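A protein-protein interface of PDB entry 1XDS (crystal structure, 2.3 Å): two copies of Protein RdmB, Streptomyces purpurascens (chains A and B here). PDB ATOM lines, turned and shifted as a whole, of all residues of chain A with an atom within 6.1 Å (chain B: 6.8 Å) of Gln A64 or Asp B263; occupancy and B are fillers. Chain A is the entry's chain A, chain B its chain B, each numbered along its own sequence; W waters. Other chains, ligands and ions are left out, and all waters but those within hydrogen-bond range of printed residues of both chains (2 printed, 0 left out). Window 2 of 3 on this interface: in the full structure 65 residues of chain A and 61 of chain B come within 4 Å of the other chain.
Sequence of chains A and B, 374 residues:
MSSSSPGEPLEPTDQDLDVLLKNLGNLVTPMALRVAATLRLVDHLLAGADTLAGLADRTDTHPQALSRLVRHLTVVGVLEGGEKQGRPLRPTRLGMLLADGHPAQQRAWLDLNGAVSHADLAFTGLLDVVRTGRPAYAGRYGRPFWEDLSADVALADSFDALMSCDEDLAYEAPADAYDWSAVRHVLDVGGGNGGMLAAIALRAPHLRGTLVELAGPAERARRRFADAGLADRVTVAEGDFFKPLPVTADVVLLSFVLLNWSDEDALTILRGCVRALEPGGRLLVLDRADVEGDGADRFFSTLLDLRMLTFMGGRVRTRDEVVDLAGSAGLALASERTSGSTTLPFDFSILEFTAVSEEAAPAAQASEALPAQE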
ATOM      1  N   LEU A  52     -17.296  -1.565  15.156  1.00  0.00           N
ATOM      2  CA  LEU A  52     -15.985  -1.824  14.575  1.00  0.00           C
ATOM      3  C   LEU A  52     -16.114  -1.965  13.061  1.00  0.00           C
ATOM      4  O   LEU A  52     -15.330  -1.393  12.305  1.00  0.00           O
ATOM      5  CB  LEU A  52     -15.402  -3.108  15.176  1.00  0.00           C
ATOM      6  CG  LEU A  52     -14.093  -3.649  14.593  1.00  0.00           C
ATOM      7  CD1 LEU A  52     -12.913  -2.852  15.140  1.00  0.00           C
ATOM      8  CD2 LEU A  52     -13.936  -5.152  14.876  1.00  0.00           C
ATOM      9  N   HIS A  62      -8.312  -2.984   7.126  1.00  0.00           N
ATOM     10  CA  HIS A  62      -8.471  -4.371   7.529  1.00  0.00           C
ATOM     11  C   HIS A  62      -9.158  -4.494   8.900  1.00  0.00           C
ATOM     12  O   HIS A  62      -8.584  -4.112   9.929  1.00  0.00           O
ATOM     13  CB  HIS A  62      -7.118  -5.054   7.586  1.00  0.00           C
ATOM     14  CG  HIS A  62      -7.195  -6.541   7.734  1.00  0.00           C
ATOM     15  ND1 HIS A  62      -6.587  -7.217   8.769  1.00  0.00           N
ATOM     16  CD2 HIS A  62      -7.774  -7.487   6.955  1.00  0.00           C
ATOM     17  CE1 HIS A  62      -6.786  -8.514   8.624  1.00  0.00           C
ATOM     18  NE2 HIS A  62      -7.506  -8.704   7.532  1.00  0.00           N
ATOM     19  N   PRO A  63     -10.376  -5.042   8.903  1.00  0.00           N
ATOM     20  CA  PRO A  63     -11.187  -5.135  10.124  1.00  0.00           C
ATOM     21  C   PRO A  63     -10.482  -5.676  11.374  1.00  0.00           C
ATOM     22  O   PRO A  63     -10.592  -5.020  12.408  1.00  0.00           O
ATOM     23  CB  PRO A  63     -12.359  -6.040   9.699  1.00  0.00           C
ATOM     24  CG  PRO A  63     -12.494  -5.780   8.200  1.00  0.00           C
ATOM     25  CD  PRO A  63     -11.092  -5.570   7.720  1.00  0.00           C
ATOM     26  N   GLN A  64      -9.800  -6.812  11.300  1.00  0.00           N
ATOM     27  CA  GLN A  64      -9.101  -7.356  12.461  1.00  0.00           C
ATOM     28  C   GLN A  64      -7.896  -6.498  12.856  1.00  0.00           C
ATOM     29  O   GLN A  64      -7.605  -6.317  14.062  1.00  0.00           O
ATOM     30  CB  GLN A  64      -8.637  -8.800  12.216  1.00  0.00           C
ATOM     31  CG  GLN A  64      -8.015  -9.479  13.462  1.00  0.00           C
ATOM     32  CD  GLN A  64      -7.439 -10.892  13.191  1.00  0.00           C
ATOM     33  OE1 GLN A  64      -6.428 -11.048  12.490  1.00  0.00           O
ATOM     34  NE2 GLN A  64      -8.074 -11.903  13.760  1.00  0.00           N
ATOM     35  N   ALA A  65      -7.185  -5.977  11.861  1.00  0.00           N
ATOM     36  CA  ALA A  65      -5.994  -5.176  12.151  1.00  0.00           C
ATOM     37  C   ALA A  65      -6.417  -3.888  12.854  1.00  0.00           C
ATOM     38  O   ALA A  65      -5.809  -3.485  13.833  1.00  0.00           O
ATOM     39  CB  ALA A  65      -5.211  -4.870  10.875  1.00  0.00           C
ATOM     40  N   LEU A  66      -7.481  -3.276  12.345  1.00  0.00           N
ATOM     41  CA  LEU A  66      -8.044  -2.065  12.907  1.00  0.00           C
ATOM     42  C   LEU A  66      -8.518  -2.262  14.340  1.00  0.00           C
ATOM     43  O   LEU A  66      -8.264  -1.404  15.200  1.00  0.00           O
ATOM     44  CB  LEU A  66      -9.215  -1.590  12.058  1.00  0.00           C
ATOM     45  CG  LEU A  66      -9.923  -0.337  12.574  1.00  0.00           C
ATOM     46  CD1 LEU A  66      -9.014   0.897  12.427  1.00  0.00           C
ATOM     47  CD2 LEU A  66     -11.234  -0.147  11.849  1.00  0.00           C
ATOM     48  N   SER A  67      -9.191  -3.385  14.601  1.00  0.00           N
ATOM     49  CA  SER A  67      -9.722  -3.666  15.938  1.00  0.00           C
ATOM     50  C   SER A  67      -8.583  -3.823  16.924  1.00  0.00           C
ATOM     51  O   SER A  67      -8.750  -3.603  18.121  1.00  0.00           O
ATOM     52  CB  SER A  67     -10.582  -4.957  15.948  1.00  0.00           C
ATOM     53  OG  SER A  67      -9.758  -6.108  15.771  1.00  0.00           O
ATOM     54  N   ARG A  68      -7.429  -4.235  16.425  1.00  0.00           N
ATOM     55  CA  ARG A  68      -6.265  -4.401  17.265  1.00  0.00           C
ATOM     56  C   ARG A  68      -5.546  -3.088  17.540  1.00  0.00           C
ATOM     57  O   ARG A  68      -4.954  -2.941  18.600  1.00  0.00           O
ATOM     58  CB  ARG A  68      -5.316  -5.405  16.652  1.00  0.00           C
ATOM     59  CG  ARG A  68      -5.850  -6.829  16.712  1.00  0.00           C
ATOM     60  CD  ARG A  68      -5.243  -7.739  15.639  1.00  0.00           C
ATOM     61  NE  ARG A  68      -3.840  -8.020  15.940  1.00  0.00           N
ATOM     62  CZ  ARG A  68      -3.084  -8.843  15.236  1.00  0.00           C
ATOM     63  NH1 ARG A  68      -3.562  -9.431  14.150  1.00  0.00           N
ATOM     64  NH2 ARG A  68      -1.834  -9.062  15.598  1.00  0.00           N
ATOM     65  N   LEU A  69      -5.604  -2.154  16.583  1.00  0.00           N
ATOM     66  CA  LEU A  69      -5.139  -0.770  16.780  1.00  0.00           C
ATOM     67  C   LEU A  69      -6.055  -0.116  17.800  1.00  0.00           C
ATOM     68  O   LEU A  69      -5.586   0.505  18.720  1.00  0.00           O
ATOM     69  CB  LEU A  69      -5.157   0.043  15.465  1.00  0.00           C
ATOM     70  CG  LEU A  69      -4.843   1.542  15.556  1.00  0.00           C
ATOM     71  CD1 LEU A  69      -3.404   1.782  15.993  1.00  0.00           C
ATOM     72  CD2 LEU A  69      -5.130   2.263  14.236  1.00  0.00           C
ATOM     73  N   VAL B 130      -2.121  -1.561   9.034  1.00  0.00           N
ATOM     74  CA  VAL B 130      -3.516  -1.501   9.454  1.00  0.00           C
ATOM     75  C   VAL B 130      -4.487  -1.501   8.271  1.00  0.00           C
ATOM     76  O   VAL B 130      -5.611  -1.974   8.409  1.00  0.00           O
ATOM     77  CB  VAL B 130      -3.768  -0.281  10.360  1.00  0.00           C
ATOM     78  CG1 VAL B 130      -5.245  -0.184  10.777  1.00  0.00           C
ATOM     79  CG2 VAL B 130      -2.867  -0.338  11.598  1.00  0.00           C
ATOM     80  N   LEU B 258       2.669 -19.808  18.711  1.00  0.00           N
ATOM     81  CA  LEU B 258       1.387 -19.496  18.072  1.00  0.00           C
ATOM     82  C   LEU B 258       1.225 -18.002  17.802  1.00  0.00           C
ATOM     83  O   LEU B 258       0.656 -17.624  16.786  1.00  0.00           O
ATOM     84  CB  LEU B 258       0.194 -20.005  18.879  1.00  0.00           C
ATOM     85  CG  LEU B 258       0.015 -21.520  18.930  1.00  0.00           C
ATOM     86  CD1 LEU B 258      -1.296 -21.837  19.650  1.00  0.00           C
ATOM     87  CD2 LEU B 258       0.078 -22.174  17.523  1.00  0.00           C
ATOM     88  N   TRP B 261       2.029 -16.321  14.336  1.00  0.00           N
ATOM     89  CA  TRP B 261       1.329 -16.716  13.130  1.00  0.00           C
ATOM     90  C   TRP B 261      -0.116 -16.242  13.129  1.00  0.00           C
ATOM     91  O   TRP B 261      -0.681 -15.935  14.170  1.00  0.00           O
ATOM     92  CB  TRP B 261       1.406 -18.245  12.979  1.00  0.00           C
ATOM     93  CG  TRP B 261       2.822 -18.715  12.973  1.00  0.00           C
ATOM     94  CD1 TRP B 261       3.509 -19.224  14.024  1.00  0.00           C
ATOM     95  CD2 TRP B 261       3.749 -18.665  11.877  1.00  0.00           C
ATOM     96  NE1 TRP B 261       4.802 -19.512  13.661  1.00  0.00           N
ATOM     97  CE2 TRP B 261       4.976 -19.184  12.343  1.00  0.00           C
ATOM     98  CE3 TRP B 261       3.667 -18.238  10.551  1.00  0.00           C
ATOM     99  CZ2 TRP B 261       6.108 -19.293  11.524  1.00  0.00           C
ATOM    100  CZ3 TRP B 261       4.788 -18.332   9.740  1.00  0.00           C
ATOM    101  CH2 TRP B 261       5.984 -18.859  10.220  1.00  0.00           C
ATOM    102  N   SER B 262      -0.685 -16.175  11.933  1.00  0.00           N
ATOM    103  CA  SER B 262      -2.078 -15.826  11.738  1.00  0.00           C
ATOM    104  C   SER B 262      -2.923 -17.028  12.101  1.00  0.00           C
ATOM    105  O   SER B 262      -2.410 -18.129  12.275  1.00  0.00           O
ATOM    106  CB  SER B 262      -2.326 -15.474  10.267  1.00  0.00           C
ATOM    107  OG  SER B 262      -2.225 -16.636   9.462  1.00  0.00           O
ATOM    108  N   ASP B 263      -4.227 -16.826  12.163  1.00  0.00           N
ATOM    109  CA  ASP B 263      -5.142 -17.900  12.530  1.00  0.00           C
ATOM    110  C   ASP B 263      -4.991 -19.140  11.659  1.00  0.00           C
ATOM    111  O   ASP B 263      -4.819 -20.242  12.163  1.00  0.00           O
ATOM    112  CB  ASP B 263      -6.576 -17.385  12.475  1.00  0.00           C
ATOM    113  CG  ASP B 263      -6.730 -16.095  13.226  1.00  0.00           C
ATOM    114  OD1 ASP B 263      -6.394 -16.117  14.426  1.00  0.00           O
ATOM    115  OD2 ASP B 263      -7.112 -15.012  12.697  1.00  0.00           O
ATOM    116  N   GLU B 264      -5.059 -18.965  10.351  1.00  0.00           N
ATOM    117  CA  GLU B 264      -4.918 -20.085   9.433  1.00  0.00           C
ATOM    118  C   GLU B 264      -3.566 -20.828   9.610  1.00  0.00           C
ATOM    119  O   GLU B 264      -3.531 -22.048   9.567  1.00  0.00           O
ATOM    120  CB  GLU B 264      -5.096 -19.582   7.982  1.00  0.00           C
ATOM    121  CG  GLU B 264      -4.989 -20.646   6.888  1.00  0.00           C
ATOM    122  CD  GLU B 264      -4.772 -20.069   5.484  1.00  0.00           C
ATOM    123  OE1 GLU B 264      -4.977 -18.846   5.277  1.00  0.00           O
ATOM    124  OE2 GLU B 264      -4.388 -20.848   4.574  1.00  0.00           O
ATOM    125  N   ASP B 265      -2.464 -20.097   9.778  1.00  0.00           N
ATOM    126  CA  ASP B 265      -1.143 -20.719   9.931  1.00  0.00           C
ATOM    127  C   ASP B 265      -0.994 -21.422  11.294  1.00  0.00           C
ATOM    128  O   ASP B 265      -0.340 -22.465  11.388  1.00  0.00           O
ATOM    129  CB  ASP B 265      -0.018 -19.687   9.777  1.00  0.00           C
ATOM    130  CG  ASP B 265       0.238 -19.275   8.319  1.00  0.00           C
ATOM    131  OD1 ASP B 265      -0.301 -19.909   7.393  1.00  0.00           O
ATOM    132  OD2 ASP B 265       0.982 -18.312   8.017  1.00  0.00           O
ATOM    133  N   ALA B 266      -1.574 -20.835  12.337  1.00  0.00           N
ATOM    134  CA  ALA B 266      -1.523 -21.391  13.687  1.00  0.00           C
ATOM    135  C   ALA B 266      -2.413 -22.615  13.743  1.00  0.00           C
ATOM    136  O   ALA B 266      -2.131 -23.559  14.466  1.00  0.00           O
ATOM    137  CB  ALA B 266      -1.976 -20.365  14.713  1.00  0.00           C
ATOM    138  N   LEU B 267      -3.481 -22.600  12.949  1.00  0.00           N
ATOM    139  CA  LEU B 267      -4.373 -23.741  12.837  1.00  0.00           C
ATOM    140  C   LEU B 267      -3.661 -24.952  12.253  1.00  0.00           C
ATOM    141  O   LEU B 267      -3.864 -26.068  12.738  1.00  0.00           O
ATOM    142  CB  LEU B 267      -5.590 -23.396  11.977  1.00  0.00           C
ATOM    143  CG  LEU B 267      -6.813 -24.306  12.099  1.00  0.00           C
ATOM    144  CD1 LEU B 267      -7.134 -24.646  13.534  1.00  0.00           C
ATOM    145  CD2 LEU B 267      -8.035 -23.647  11.440  1.00  0.00           C
ATOM    146  N   THR B 268      -2.820 -24.756  11.237  1.00  0.00           N
ATOM    147  CA  THR B 268      -2.137 -25.902  10.639  1.00  0.00           C
ATOM    148  C   THR B 268      -0.947 -26.403  11.500  1.00  0.00           C
ATOM    149  O   THR B 268      -0.620 -27.582  11.457  1.00  0.00           O
ATOM    150  CB  THR B 268      -1.782 -25.710   9.101  1.00  0.00           C
ATOM    151  OG1 THR B 268      -0.368 -25.584   8.887  1.00  0.00           O
ATOM    152  CG2 THR B 268      -2.399 -24.454   8.486  1.00  0.00           C
ATOM    153  N   ASP B 305       1.064  -7.539  20.825  1.00  0.00           N
ATOM    154  CA  ASP B 305       0.156  -7.832  19.731  1.00  0.00           C
ATOM    155  C   ASP B 305       0.467  -7.028  18.470  1.00  0.00           C
ATOM    156  O   ASP B 305       0.380  -7.555  17.368  1.00  0.00           O
ATOM    157  CB  ASP B 305      -1.291  -7.546  20.132  1.00  0.00           C
ATOM    158  CG  ASP B 305      -2.265  -7.940  19.059  1.00  0.00           C
ATOM    159  OD1 ASP B 305      -2.196  -9.103  18.590  1.00  0.00           O
ATOM    160  OD2 ASP B 305      -3.123  -7.169  18.597  1.00  0.00           O
ATOM    161  N   LEU B 309       1.921  -8.299  14.821  1.00  0.00           N
ATOM    162  CA  LEU B 309       1.254  -7.906  13.590  1.00  0.00           C
ATOM    163  C   LEU B 309       2.257  -7.245  12.626  1.00  0.00           C
ATOM    164  O   LEU B 309       2.283  -7.540  11.423  1.00  0.00           O
ATOM    165  CB  LEU B 309       0.138  -6.913  13.897  1.00  0.00           C
ATOM    166  CG  LEU B 309      -0.571  -6.364  12.667  1.00  0.00           C
ATOM    167  CD1 LEU B 309      -1.068  -7.502  11.806  1.00  0.00           C
ATOM    168  CD2 LEU B 309      -1.703  -5.417  13.045  1.00  0.00           C
ATOM    169  N   GLY B 313       3.070 -10.503  10.952  1.00  0.00           N
ATOM    170  CA  GLY B 313       1.667 -10.847  10.768  1.00  0.00           C
ATOM    171  C   GLY B 313       1.096 -11.895  11.721  1.00  0.00           C
ATOM    172  O   GLY B 313       0.095 -12.539  11.412  1.00  0.00           O
ATOM    173  N   GLY B 314       1.719 -12.053  12.891  1.00  0.00           N
ATOM    174  CA  GLY B 314       1.209 -12.925  13.944  1.00  0.00           C
ATOM    175  C   GLY B 314       0.195 -12.210  14.807  1.00  0.00           C
ATOM    176  O   GLY B 314      -0.160 -11.089  14.494  1.00  0.00           O
ATOM    177  N   ARG B 315      -0.294 -12.855  15.866  1.00  0.00           N
ATOM    178  CA  ARG B 315      -1.168 -12.190  16.812  1.00  0.00           C
ATOM    179  C   ARG B 315      -1.184 -12.800  18.210  1.00  0.00           C
ATOM    180  O   ARG B 315      -1.181 -14.019  18.384  1.00  0.00           O
ATOM    181  CB  ARG B 315      -2.588 -12.118  16.274  1.00  0.00           C
ATOM    182  CG  ARG B 315      -3.310 -13.452  16.056  1.00  0.00           C
ATOM    183  CD  ARG B 315      -4.845 -13.324  15.931  1.00  0.00           C
ATOM    184  NE  ARG B 315      -5.428 -12.450  16.959  1.00  0.00           N
ATOM    185  CZ  ARG B 315      -6.666 -12.561  17.465  1.00  0.00           C
ATOM    186  NH1 ARG B 315      -7.510 -13.513  17.058  1.00  0.00           N
ATOM    187  NH2 ARG B 315      -7.063 -11.698  18.396  1.00  0.00           N
ATOM    188  N   ARG B 317      -3.103 -13.806  21.356  1.00  0.00           N
ATOM    189  CA  ARG B 317      -4.471 -14.312  21.472  1.00  0.00           C
ATOM    190  C   ARG B 317      -4.820 -14.436  22.946  1.00  0.00           C
ATOM    191  O   ARG B 317      -3.934 -14.676  23.763  1.00  0.00           O
ATOM    192  CB  ARG B 317      -4.600 -15.654  20.735  1.00  0.00           C
ATOM    193  CG  ARG B 317      -5.122 -15.516  19.331  1.00  0.00           C
ATOM    194  CD  ARG B 317      -5.070 -16.796  18.496  1.00  0.00           C
ATOM    195  NE  ARG B 317      -3.692 -17.101  18.214  1.00  0.00           N
ATOM    196  CZ  ARG B 317      -3.089 -16.978  17.046  1.00  0.00           C
ATOM    197  NH1 ARG B 317      -3.721 -16.621  15.937  1.00  0.00           N
ATOM    198  NH2 ARG B 317      -1.810 -17.250  16.989  1.00  0.00           N
ATOM    199  N   GLU B 321      -9.624 -17.318  22.911  1.00  0.00           N
ATOM    200  CA  GLU B 321      -9.352 -17.426  21.471  1.00  0.00           C
ATOM    201  C   GLU B 321      -8.446 -18.620  21.156  1.00  0.00           C
ATOM    202  O   GLU B 321      -8.616 -19.287  20.133  1.00  0.00           O
ATOM    203  CB  GLU B 321      -8.757 -16.124  20.947  1.00  0.00           C
ATOM    204  CG  GLU B 321      -9.703 -14.933  21.111  1.00  0.00           C
ATOM    205  CD  GLU B 321      -9.037 -13.593  20.795  1.00  0.00           C
ATOM    206  OE1 GLU B 321      -9.622 -12.816  20.020  1.00  0.00           O
ATOM    207  OE2 GLU B 321      -7.940 -13.317  21.321  1.00  0.00           O
ATOM    208  N   LEU B 325      -9.412 -21.843  18.834  1.00  0.00           N
ATOM    209  CA  LEU B 325      -8.565 -22.327  17.746  1.00  0.00           C
ATOM    210  C   LEU B 325      -8.148 -23.792  17.970  1.00  0.00           C
ATOM    211  O   LEU B 325      -8.068 -24.570  17.024  1.00  0.00           O
ATOM    212  CB  LEU B 325      -7.329 -21.435  17.607  1.00  0.00           C
ATOM    213  CG  LEU B 325      -6.591 -21.443  16.267  1.00  0.00           C
ATOM    214  CD1 LEU B 325      -7.388 -20.708  15.187  1.00  0.00           C
ATOM    215  CD2 LEU B 325      -5.213 -20.811  16.457  1.00  0.00           C
HETATM  216  O   HOH W   1      -3.886  -4.962  19.876  1.00  0.00           O
HETATM  217  O   HOH W   2      -2.341 -11.307  11.920  1.00  0.00           O
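Hydrophobic or aromatic side chains of chain B that line the printed part of chain A: Val B130 and Leu B309. Hydrophobic or aromatic side chains of chain A that line the printed part of chain B: His A62 and Ala A65. Among the printed residues, 9 pairs touch across the chains.
No position is printed for both chains. Of the 9 pairs that touch across the chains among the printed residues, none has its exchanged pair printed and touching as well.
The guanidinium group (NH2) of Arg B315 is in salt-bridge range of the side-chain carboxylate (OE1) of Glu B321. O of Gly B314 lies within hydrogen-bond range of N of Leu B309 (3.5 Å). The side-chain carboxylate (OD1) of Asp B263 is in salt-bridge range of the guanidinium group (NH1) of Arg B317, 3.1 Å away. NH1 of Arg B315 lies within salt-bridge range of OD1 of Asp B263 (3.9 Å). The backbone carbonyl oxygen (O) of Gln A64 lies within hydrogen-bond range of the side-chain hydroxyl (OG) of Ser A67, at 2.8 Å. The backbone NH (N) of Ala A65 is in hydrogen-bond range of a ring nitrogen (ND1) of His A62, 3.4 Å away.
Gln A64 touches two residues of chain B. Of chain A, only Gln A64 comes within 4 Å of Asp B263. Of the printed residues of chain A, Asp B305 touches Arg A68 (2.9 Å). Printed residues of chain B within 4 Å of His A62: Val B130 (3.2 Å). Printed residues of chain B within 4 Å of Leu A66: Val B130. Of the printed residues of chain A, Leu B309 touches Arg A68. Of the printed residues of chain A, Val B130 touches His A62 (3.2 Å), Ala A65 (3.8 Å) and Leu A66 (3.99 Å). Glu B321 touches none of the printed residues of chain A. Gly B313 touches none of the printed residues of chain A. The nearest residue of chain B that does not touch Gln A64 is Leu B309 (6.1 Å). The nearest printed residue of chain B that does not touch Arg A68 is Gly B313 (5.5 Å).
Water W1 bridges O of Arg A68 (2.6 Å) and OD2 of Asp B305 (2.7 Å). Water W2 lies within hydrogen-bond range of O of Gly B313 (2.8 Å), NH1 of Arg A68 (3.2 Å) and O of Gly B314 (3.4 Å).
The guanidinium group (NH2) of Arg A68 sits at hydrogen-bond distance from the backbone carbonyl oxygen (O) of Gly B314, 2.9 Å away. The guanidinium group (NE) of Arg A68 is in salt-bridge range of the side-chain carboxylate (OD2) of Asp B305 (2.9 Å). The backbone carbonyl oxygen (O) of Val B130 lies within hydrogen-bond range of the backbone NH (N) of His A62 (3.2 Å). OD2 of Asp B263 is in hydrogen-bond range of NE2 of Gln A64, 3.4 Å away.
Arg B315 touches Gln A64 (NH1 to NE2, 3.7 Å). CB of Ala A65 touches O of Val B130 (3.8 Å). Leu A66 touches Val B130. CB of Leu B309 touches NH2 of Arg A68, 3.4 Å away. Arg A68 touches Arg B315 (NH2 to CB, 3.2 Å).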
